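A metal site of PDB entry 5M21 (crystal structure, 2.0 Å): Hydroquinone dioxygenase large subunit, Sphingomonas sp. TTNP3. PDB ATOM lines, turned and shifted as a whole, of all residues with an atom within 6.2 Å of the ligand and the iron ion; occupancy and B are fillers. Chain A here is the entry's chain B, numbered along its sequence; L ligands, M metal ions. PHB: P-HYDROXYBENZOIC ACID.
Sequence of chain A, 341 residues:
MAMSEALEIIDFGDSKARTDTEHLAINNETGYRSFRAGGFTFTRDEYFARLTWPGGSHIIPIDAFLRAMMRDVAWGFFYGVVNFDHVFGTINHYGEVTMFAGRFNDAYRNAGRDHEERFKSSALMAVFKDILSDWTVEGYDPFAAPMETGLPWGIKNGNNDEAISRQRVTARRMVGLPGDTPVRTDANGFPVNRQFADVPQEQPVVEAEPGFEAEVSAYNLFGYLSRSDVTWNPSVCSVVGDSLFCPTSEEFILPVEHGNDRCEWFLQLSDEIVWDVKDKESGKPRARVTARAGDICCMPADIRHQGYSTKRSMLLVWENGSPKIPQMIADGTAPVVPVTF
Residues that only touch the ligand: Trp 75, Phe 78, Trp 232, Pro 234, Thr 248, Leu 254, Phe 266, Trp 275, Leu 315 and Val 317. The nearest printed residue that does not touch the ligand is Glu 319 (5.1 Å).
OE2 of Glu 250 sits at hydrogen-bond distance from O4 of the ligand. An oxygen (O4) of the ligand is in hydrogen-bond range of the backbone NH (N) of Asn 233 (3.3 Å).
ND1 of His 305 is in hydrogen-bond range of SD of Met 299 (3.7 Å). The side-chain carboxylate (OE2) of Glu 264 lies close to the side-chain amide nitrogen (ND2) of Asn 260. OE1 of Glu 250 sits at hydrogen-bond distance from N of Trp 232 (3.0 Å). The side-chain carboxylate (OE1) of Glu 250 is in hydrogen-bond range of the side-chain hydroxyl (OG1) of Thr 248 (2.9 Å). The backbone NH of Trp 232 sits at hydrogen-bond distance from the backbone carbonyl oxygen of Ser 249 (3.1 Å). The side-chain hydroxyl of Thr 248 lies within hydrogen-bond range of the backbone NH of Asn 233, 2.8 Å away. The indole nitrogen (NE1) of Trp 75 lies within hydrogen-bond range of the side-chain amide oxygen (OD1) of Asn 233 (2.9 Å). O of Thr 248 sits at hydrogen-bond distance from N of Leu 315, 2.9 Å away.
Three residues have an atom within 4 Å of the iron ion: His 258, Glu 264 and His 305. Along chain A the residues within 4 Å of the iron ion span positions 258 to 305. The nearest printed residue that does not touch the iron ion is Phe 266 (4.1 Å).
O1' of the ligand is bound to the iron ion. ND1 of His 258 binds the iron ion. NE2 of His 305 binds the iron ion, at 2.2 Å. OE2 of Glu 264 binds the iron ion, at 2.2 Å. O2' of the ligand binds the iron ion (2.3 Å). Slightly farther from the iron ion lies OE1 of Glu 264 (2.6 Å).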
ATOM      1  N   TRP A  75       6.072   3.119   6.148  1.00  0.00           N
ATOM      2  CA  TRP A  75       5.536   4.488   6.239  1.00  0.00           C
ATOM      3  C   TRP A  75       4.732   4.736   7.500  1.00  0.00           C
ATOM      4  O   TRP A  75       4.106   5.814   7.624  1.00  0.00           O
ATOM      5  CB  TRP A  75       4.667   4.868   5.015  1.00  0.00           C
ATOM      6  CG  TRP A  75       5.239   4.626   3.653  1.00  0.00           C
ATOM      7  CD1 TRP A  75       6.586   4.607   3.289  1.00  0.00           C
ATOM      8  CD2 TRP A  75       4.504   4.473   2.428  1.00  0.00           C
ATOM      9  NE1 TRP A  75       6.707   4.392   1.933  1.00  0.00           N
ATOM     10  CE2 TRP A  75       5.455   4.328   1.376  1.00  0.00           C
ATOM     11  CE3 TRP A  75       3.132   4.373   2.126  1.00  0.00           C
ATOM     12  CZ2 TRP A  75       5.078   4.100   0.041  1.00  0.00           C
ATOM     13  CZ3 TRP A  75       2.753   4.151   0.784  1.00  0.00           C
ATOM     14  CH2 TRP A  75       3.731   3.983  -0.240  1.00  0.00           C
ATOM     15  N   PHE A  78       1.374   5.810   6.521  1.00  0.00           N
ATOM     16  CA  PHE A  78       1.450   6.958   5.606  1.00  0.00           C
ATOM     17  C   PHE A  78       0.411   8.061   5.927  1.00  0.00           C
ATOM     18  O   PHE A  78       0.142   8.320   7.093  1.00  0.00           O
ATOM     19  CB  PHE A  78       1.249   6.427   4.208  1.00  0.00           C
ATOM     20  CG  PHE A  78       1.968   7.206   3.174  1.00  0.00           C
ATOM     21  CD1 PHE A  78       3.192   7.841   3.466  1.00  0.00           C
ATOM     22  CD2 PHE A  78       1.467   7.275   1.874  1.00  0.00           C
ATOM     23  CE1 PHE A  78       3.881   8.571   2.501  1.00  0.00           C
ATOM     24  CE2 PHE A  78       2.152   7.997   0.902  1.00  0.00           C
ATOM     25  CZ  PHE A  78       3.352   8.646   1.211  1.00  0.00           C
ATOM     26  N   THR A 231      12.715   1.319  -3.359  1.00  0.00           N
ATOM     27  CA  THR A 231      11.921   1.921  -4.407  1.00  0.00           C
ATOM     28  C   THR A 231      10.648   2.446  -3.757  1.00  0.00           C
ATOM     29  O   THR A 231      10.185   1.879  -2.731  1.00  0.00           O
ATOM     30  CB  THR A 231      11.604   0.954  -5.547  1.00  0.00           C
ATOM     31  OG1 THR A 231      10.870  -0.204  -5.043  1.00  0.00           O
ATOM     32  CG2 THR A 231      12.889   0.481  -6.167  1.00  0.00           C
ATOM     33  N   TRP A 232      10.078   3.507  -4.293  1.00  0.00           N
ATOM     34  CA  TRP A 232       8.769   3.973  -3.792  1.00  0.00           C
ATOM     35  C   TRP A 232       8.760   4.189  -2.283  1.00  0.00           C
ATOM     36  O   TRP A 232       7.970   3.577  -1.545  1.00  0.00           O
ATOM     37  CB  TRP A 232       7.632   3.063  -4.176  1.00  0.00           C
ATOM     38  CG  TRP A 232       7.625   2.748  -5.634  1.00  0.00           C
ATOM     39  CD1 TRP A 232       8.072   1.601  -6.223  1.00  0.00           C
ATOM     40  CD2 TRP A 232       7.078   3.585  -6.696  1.00  0.00           C
ATOM     41  NE1 TRP A 232       7.813   1.651  -7.593  1.00  0.00           N
ATOM     42  CE2 TRP A 232       7.227   2.855  -7.912  1.00  0.00           C
ATOM     43  CE3 TRP A 232       6.498   4.865  -6.726  1.00  0.00           C
ATOM     44  CZ2 TRP A 232       6.842   3.387  -9.168  1.00  0.00           C
ATOM     45  CZ3 TRP A 232       6.084   5.384  -7.962  1.00  0.00           C
ATOM     46  CH2 TRP A 232       6.274   4.646  -9.179  1.00  0.00           C
ATOM     47  N   ASN A 233       9.605   5.112  -1.840  1.00  0.00           N
ATOM     48  CA  ASN A 233       9.769   5.383  -0.432  1.00  0.00           C
ATOM     49  C   ASN A 233      10.123   6.859  -0.163  1.00  0.00           C
ATOM     50  O   ASN A 233      11.303   7.203   0.023  1.00  0.00           O
ATOM     51  CB  ASN A 233      10.806   4.444   0.195  1.00  0.00           C
ATOM     52  CG  ASN A 233      10.732   4.476   1.705  1.00  0.00           C
ATOM     53  OD1 ASN A 233       9.631   4.401   2.291  1.00  0.00           O
ATOM     54  ND2 ASN A 233      11.871   4.611   2.354  1.00  0.00           N
ATOM     55  N   PRO A 234       9.101   7.745  -0.214  1.00  0.00           N
ATOM     56  CA  PRO A 234       9.261   9.170   0.005  1.00  0.00           C
ATOM     57  C   PRO A 234       9.964   9.369   1.352  1.00  0.00           C
ATOM     58  O   PRO A 234       9.542   8.794   2.378  1.00  0.00           O
ATOM     59  CB  PRO A 234       7.820   9.660   0.137  1.00  0.00           C
ATOM     60  CG  PRO A 234       7.020   8.668  -0.638  1.00  0.00           C
ATOM     61  CD  PRO A 234       7.687   7.371  -0.306  1.00  0.00           C
ATOM     62  N   THR A 248      12.376  10.324  -3.700  1.00  0.00           N
ATOM     63  CA  THR A 248      12.512   8.859  -3.659  1.00  0.00           C
ATOM     64  C   THR A 248      12.866   8.406  -5.058  1.00  0.00           C
ATOM     65  O   THR A 248      12.628   9.168  -6.038  1.00  0.00           O
ATOM     66  CB  THR A 248      11.164   8.180  -3.201  1.00  0.00           C
ATOM     67  OG1 THR A 248      11.192   6.770  -3.425  1.00  0.00           O
ATOM     68  CG2 THR A 248       9.961   8.744  -3.973  1.00  0.00           C
ATOM     69  N   SER A 249      13.461   7.227  -5.170  1.00  0.00           N
ATOM     70  CA  SER A 249      13.641   6.620  -6.499  1.00  0.00           C
ATOM     71  C   SER A 249      12.637   5.504  -6.775  1.00  0.00           C
ATOM     72  O   SER A 249      12.466   4.582  -5.968  1.00  0.00           O
ATOM     73  CB  SER A 249      15.063   6.109  -6.698  1.00  0.00           C
ATOM     74  OG  SER A 249      15.357   5.085  -5.753  1.00  0.00           O
ATOM     75  N   GLU A 250      12.066   5.527  -7.969  1.00  0.00           N
ATOM     76  CA  GLU A 250      10.878   4.752  -8.281  1.00  0.00           C
ATOM     77  C   GLU A 250      11.165   3.770  -9.404  1.00  0.00           C
ATOM     78  O   GLU A 250      11.692   4.147 -10.404  1.00  0.00           O
ATOM     79  CB  GLU A 250       9.788   5.696  -8.789  1.00  0.00           C
ATOM     80  CG  GLU A 250       9.598   7.016  -8.031  1.00  0.00           C
ATOM     81  CD  GLU A 250       9.202   6.821  -6.593  1.00  0.00           C
ATOM     82  OE1 GLU A 250       9.947   6.069  -5.903  1.00  0.00           O
ATOM     83  OE2 GLU A 250       8.161   7.401  -6.121  1.00  0.00           O
ATOM     84  N   LEU A 254       4.267   1.447  -8.144  1.00  0.00           N
ATOM     85  CA  LEU A 254       3.949   1.787  -6.781  1.00  0.00           C
ATOM     86  C   LEU A 254       3.078   0.663  -6.226  1.00  0.00           C
ATOM     87  O   LEU A 254       2.000   0.397  -6.746  1.00  0.00           O
ATOM     88  CB  LEU A 254       3.194   3.130  -6.702  1.00  0.00           C
ATOM     89  CG  LEU A 254       2.797   3.533  -5.298  1.00  0.00           C
ATOM     90  CD1 LEU A 254       4.000   3.570  -4.385  1.00  0.00           C
ATOM     91  CD2 LEU A 254       2.201   4.932  -5.330  1.00  0.00           C
ATOM     92  N   VAL A 256       1.060   0.347  -3.928  1.00  0.00           N
ATOM     93  CA  VAL A 256      -0.292   0.674  -3.393  1.00  0.00           C
ATOM     94  C   VAL A 256      -1.012   1.689  -4.301  1.00  0.00           C
ATOM     95  O   VAL A 256      -0.378   2.272  -5.144  1.00  0.00           O
ATOM     96  CB  VAL A 256      -0.203   1.212  -1.944  1.00  0.00           C
ATOM     97  CG1 VAL A 256       0.507   0.217  -1.018  1.00  0.00           C
ATOM     98  CG2 VAL A 256       0.542   2.534  -1.938  1.00  0.00           C
ATOM     99  N   HIS A 258      -2.632   5.085  -3.518  1.00  0.00           N
ATOM    100  CA  HIS A 258      -2.688   6.048  -2.437  1.00  0.00           C
ATOM    101  C   HIS A 258      -3.883   7.000  -2.616  1.00  0.00           C
ATOM    102  O   HIS A 258      -3.933   7.744  -3.576  1.00  0.00           O
ATOM    103  CB  HIS A 258      -1.368   6.827  -2.329  1.00  0.00           C
ATOM    104  CG  HIS A 258      -1.321   7.715  -1.131  1.00  0.00           C
ATOM    105  ND1 HIS A 258      -0.631   8.912  -1.103  1.00  0.00           N
ATOM    106  CD2 HIS A 258      -1.992   7.644   0.048  1.00  0.00           C
ATOM    107  CE1 HIS A 258      -0.842   9.516   0.055  1.00  0.00           C
ATOM    108  NE2 HIS A 258      -1.664   8.760   0.770  1.00  0.00           N
ATOM    109  N   GLY A 259      -4.806   6.996  -1.655  1.00  0.00           N
ATOM    110  CA  GLY A 259      -5.847   8.013  -1.579  1.00  0.00           C
ATOM    111  C   GLY A 259      -5.570   8.955  -0.414  1.00  0.00           C
ATOM    112  O   GLY A 259      -5.837   8.632   0.747  1.00  0.00           O
ATOM    113  N   ASN A 260      -5.009  10.109  -0.705  1.00  0.00           N
ATOM    114  CA  ASN A 260      -4.489  10.948   0.358  1.00  0.00           C
ATOM    115  C   ASN A 260      -5.654  11.649   1.006  1.00  0.00           C
ATOM    116  O   ASN A 260      -6.766  11.681   0.441  1.00  0.00           O
ATOM    117  CB  ASN A 260      -3.393  11.851  -0.185  1.00  0.00           C
ATOM    118  CG  ASN A 260      -2.415  12.307   0.884  1.00  0.00           C
ATOM    119  OD1 ASN A 260      -2.733  12.301   2.058  1.00  0.00           O
ATOM    120  ND2 ASN A 260      -1.231  12.777   0.474  1.00  0.00           N
ATOM    121  N   GLU A 264      -1.517  16.583  -2.554  1.00  0.00           N
ATOM    122  CA  GLU A 264      -0.093  16.381  -2.623  1.00  0.00           C
ATOM    123  C   GLU A 264       0.402  16.626  -4.035  1.00  0.00           C
ATOM    124  O   GLU A 264      -0.365  16.591  -4.981  1.00  0.00           O
ATOM    125  CB  GLU A 264       0.273  14.965  -2.143  1.00  0.00           C
ATOM    126  CG  GLU A 264       0.194  13.881  -3.185  1.00  0.00           C
ATOM    127  CD  GLU A 264       0.330  12.520  -2.565  1.00  0.00           C
ATOM    128  OE1 GLU A 264       1.438  12.135  -2.194  1.00  0.00           O
ATOM    129  OE2 GLU A 264      -0.698  11.873  -2.386  1.00  0.00           O
ATOM    130  N   PHE A 266       3.674  16.185  -7.059  1.00  0.00           N
ATOM    131  CA  PHE A 266       4.729  15.309  -7.599  1.00  0.00           C
ATOM    132  C   PHE A 266       5.551  16.135  -8.532  1.00  0.00           C
ATOM    133  O   PHE A 266       4.995  16.757  -9.484  1.00  0.00           O
ATOM    134  CB  PHE A 266       4.159  14.171  -8.485  1.00  0.00           C
ATOM    135  CG  PHE A 266       3.357  13.130  -7.712  1.00  0.00           C
ATOM    136  CD1 PHE A 266       3.630  12.863  -6.370  1.00  0.00           C
ATOM    137  CD2 PHE A 266       2.329  12.418  -8.341  1.00  0.00           C
ATOM    138  CE1 PHE A 266       2.897  11.887  -5.659  1.00  0.00           C
ATOM    139  CE2 PHE A 266       1.598  11.456  -7.632  1.00  0.00           C
ATOM    140  CZ  PHE A 266       1.889  11.185  -6.297  1.00  0.00           C
ATOM    141  N   TRP A 275       1.016   8.071 -14.030  1.00  0.00           N
ATOM    142  CA  TRP A 275       0.146   7.858 -12.885  1.00  0.00           C
ATOM    143  C   TRP A 275      -1.246   7.406 -13.337  1.00  0.00           C
ATOM    144  O   TRP A 275      -1.875   8.112 -14.153  1.00  0.00           O
ATOM    145  CB  TRP A 275       0.037   9.169 -12.082  1.00  0.00           C
ATOM    146  CG  TRP A 275       1.359   9.586 -11.501  1.00  0.00           C
ATOM    147  CD1 TRP A 275       2.263  10.484 -12.029  1.00  0.00           C
ATOM    148  CD2 TRP A 275       1.936   9.093 -10.284  1.00  0.00           C
ATOM    149  NE1 TRP A 275       3.361  10.586 -11.202  1.00  0.00           N
ATOM    150  CE2 TRP A 275       3.207   9.711 -10.146  1.00  0.00           C
ATOM    151  CE3 TRP A 275       1.524   8.152  -9.320  1.00  0.00           C
ATOM    152  CZ2 TRP A 275       4.066   9.452  -9.056  1.00  0.00           C
ATOM    153  CZ3 TRP A 275       2.374   7.895  -8.227  1.00  0.00           C
ATOM    154  CH2 TRP A 275       3.640   8.539  -8.119  1.00  0.00           C
ATOM    155  N   MET A 299      -2.000  15.894  -7.071  1.00  0.00           N
ATOM    156  CA  MET A 299      -3.039  14.870  -6.944  1.00  0.00           C
ATOM    157  C   MET A 299      -4.139  15.419  -6.052  1.00  0.00           C
ATOM    158  O   MET A 299      -3.917  15.688  -4.895  1.00  0.00           O
ATOM    159  CB  MET A 299      -2.492  13.579  -6.322  1.00  0.00           C
ATOM    160  CG  MET A 299      -1.382  12.995  -7.194  1.00  0.00           C
ATOM    161  SD  MET A 299      -2.171  12.175  -8.578  1.00  0.00           S
ATOM    162  CE  MET A 299      -1.312  12.944  -9.963  1.00  0.00           C
ATOM    163  N   HIS A 305      -4.101   7.183  -6.422  1.00  0.00           N
ATOM    164  CA  HIS A 305      -3.194   7.091  -7.568  1.00  0.00           C
ATOM    165  C   HIS A 305      -2.170   6.005  -7.382  1.00  0.00           C
ATOM    166  O   HIS A 305      -1.826   5.677  -6.223  1.00  0.00           O
ATOM    167  CB  HIS A 305      -2.457   8.396  -7.748  1.00  0.00           C
ATOM    168  CG  HIS A 305      -2.018   8.992  -6.454  1.00  0.00           C
ATOM    169  ND1 HIS A 305      -2.802   9.870  -5.746  1.00  0.00           N
ATOM    170  CD2 HIS A 305      -0.896   8.806  -5.731  1.00  0.00           C
ATOM    171  CE1 HIS A 305      -2.190  10.183  -4.630  1.00  0.00           C
ATOM    172  NE2 HIS A 305      -1.025   9.564  -4.600  1.00  0.00           N
ATOM    173  N   LEU A 315      11.885  11.061  -8.154  1.00  0.00           N
ATOM    174  CA  LEU A 315      10.659  11.792  -8.038  1.00  0.00           C
ATOM    175  C   LEU A 315      10.724  12.616  -6.752  1.00  0.00           C
ATOM    176  O   LEU A 315      11.264  12.160  -5.775  1.00  0.00           O
ATOM    177  CB  LEU A 315       9.525  10.778  -7.967  1.00  0.00           C
ATOM    178  CG  LEU A 315       8.154  11.386  -7.574  1.00  0.00           C
ATOM    179  CD1 LEU A 315       7.597  12.207  -8.714  1.00  0.00           C
ATOM    180  CD2 LEU A 315       7.188  10.279  -7.227  1.00  0.00           C
ATOM    181  N   VAL A 317       8.222  13.976  -3.978  1.00  0.00           N
ATOM    182  CA  VAL A 317       6.832  13.987  -3.521  1.00  0.00           C
ATOM    183  C   VAL A 317       6.734  15.164  -2.515  1.00  0.00           C
ATOM    184  O   VAL A 317       7.457  15.187  -1.558  1.00  0.00           O
ATOM    185  CB  VAL A 317       6.452  12.648  -2.861  1.00  0.00           C
ATOM    186  CG1 VAL A 317       5.029  12.737  -2.305  1.00  0.00           C
ATOM    187  CG2 VAL A 317       6.559  11.505  -3.865  1.00  0.00           C
ATOM    188  N   GLU A 319       4.656  17.269   0.331  1.00  0.00           N
ATOM    189  CA  GLU A 319       3.583  17.076   1.303  1.00  0.00           C
ATOM    190  C   GLU A 319       3.428  18.285   2.253  1.00  0.00           C
ATOM    191  O   GLU A 319       4.384  18.959   2.624  1.00  0.00           O
ATOM    192  CB  GLU A 319       3.850  15.821   2.176  1.00  0.00           C
ATOM    193  CG  GLU A 319       3.880  14.491   1.436  1.00  0.00           C
ATOM    194  CD  GLU A 319       2.493  13.833   1.071  1.00  0.00           C
ATOM    195  OE1 GLU A 319       2.566  12.772   0.394  1.00  0.00           O
ATOM    196  OE2 GLU A 319       1.333  14.258   1.471  1.00  0.00           O
HETATM  197  C1' PHB L   1       2.309   8.573  -3.176  1.00  0.00           C
HETATM  198  O1' PHB L   1       2.089   9.700  -3.610  1.00  0.00           O
HETATM  199  O2' PHB L   1       1.547   7.974  -2.404  1.00  0.00           O
HETATM  200  C1  PHB L   1       3.633   7.949  -3.481  1.00  0.00           C
HETATM  201  C2  PHB L   1       4.493   8.528  -4.420  1.00  0.00           C
HETATM  202  C3  PHB L   1       5.778   8.040  -4.590  1.00  0.00           C
HETATM  203  C4  PHB L   1       6.222   6.979  -3.807  1.00  0.00           C
HETATM  204  C5  PHB L   1       5.375   6.395  -2.889  1.00  0.00           C
HETATM  205  C6  PHB L   1       4.082   6.869  -2.730  1.00  0.00           C
HETATM  206  O4  PHB L   1       7.488   6.516  -3.926  1.00  0.00           O
HETATM  207 FE    FE M   1       0.236   9.869  -2.793  1.00  0.00          FE
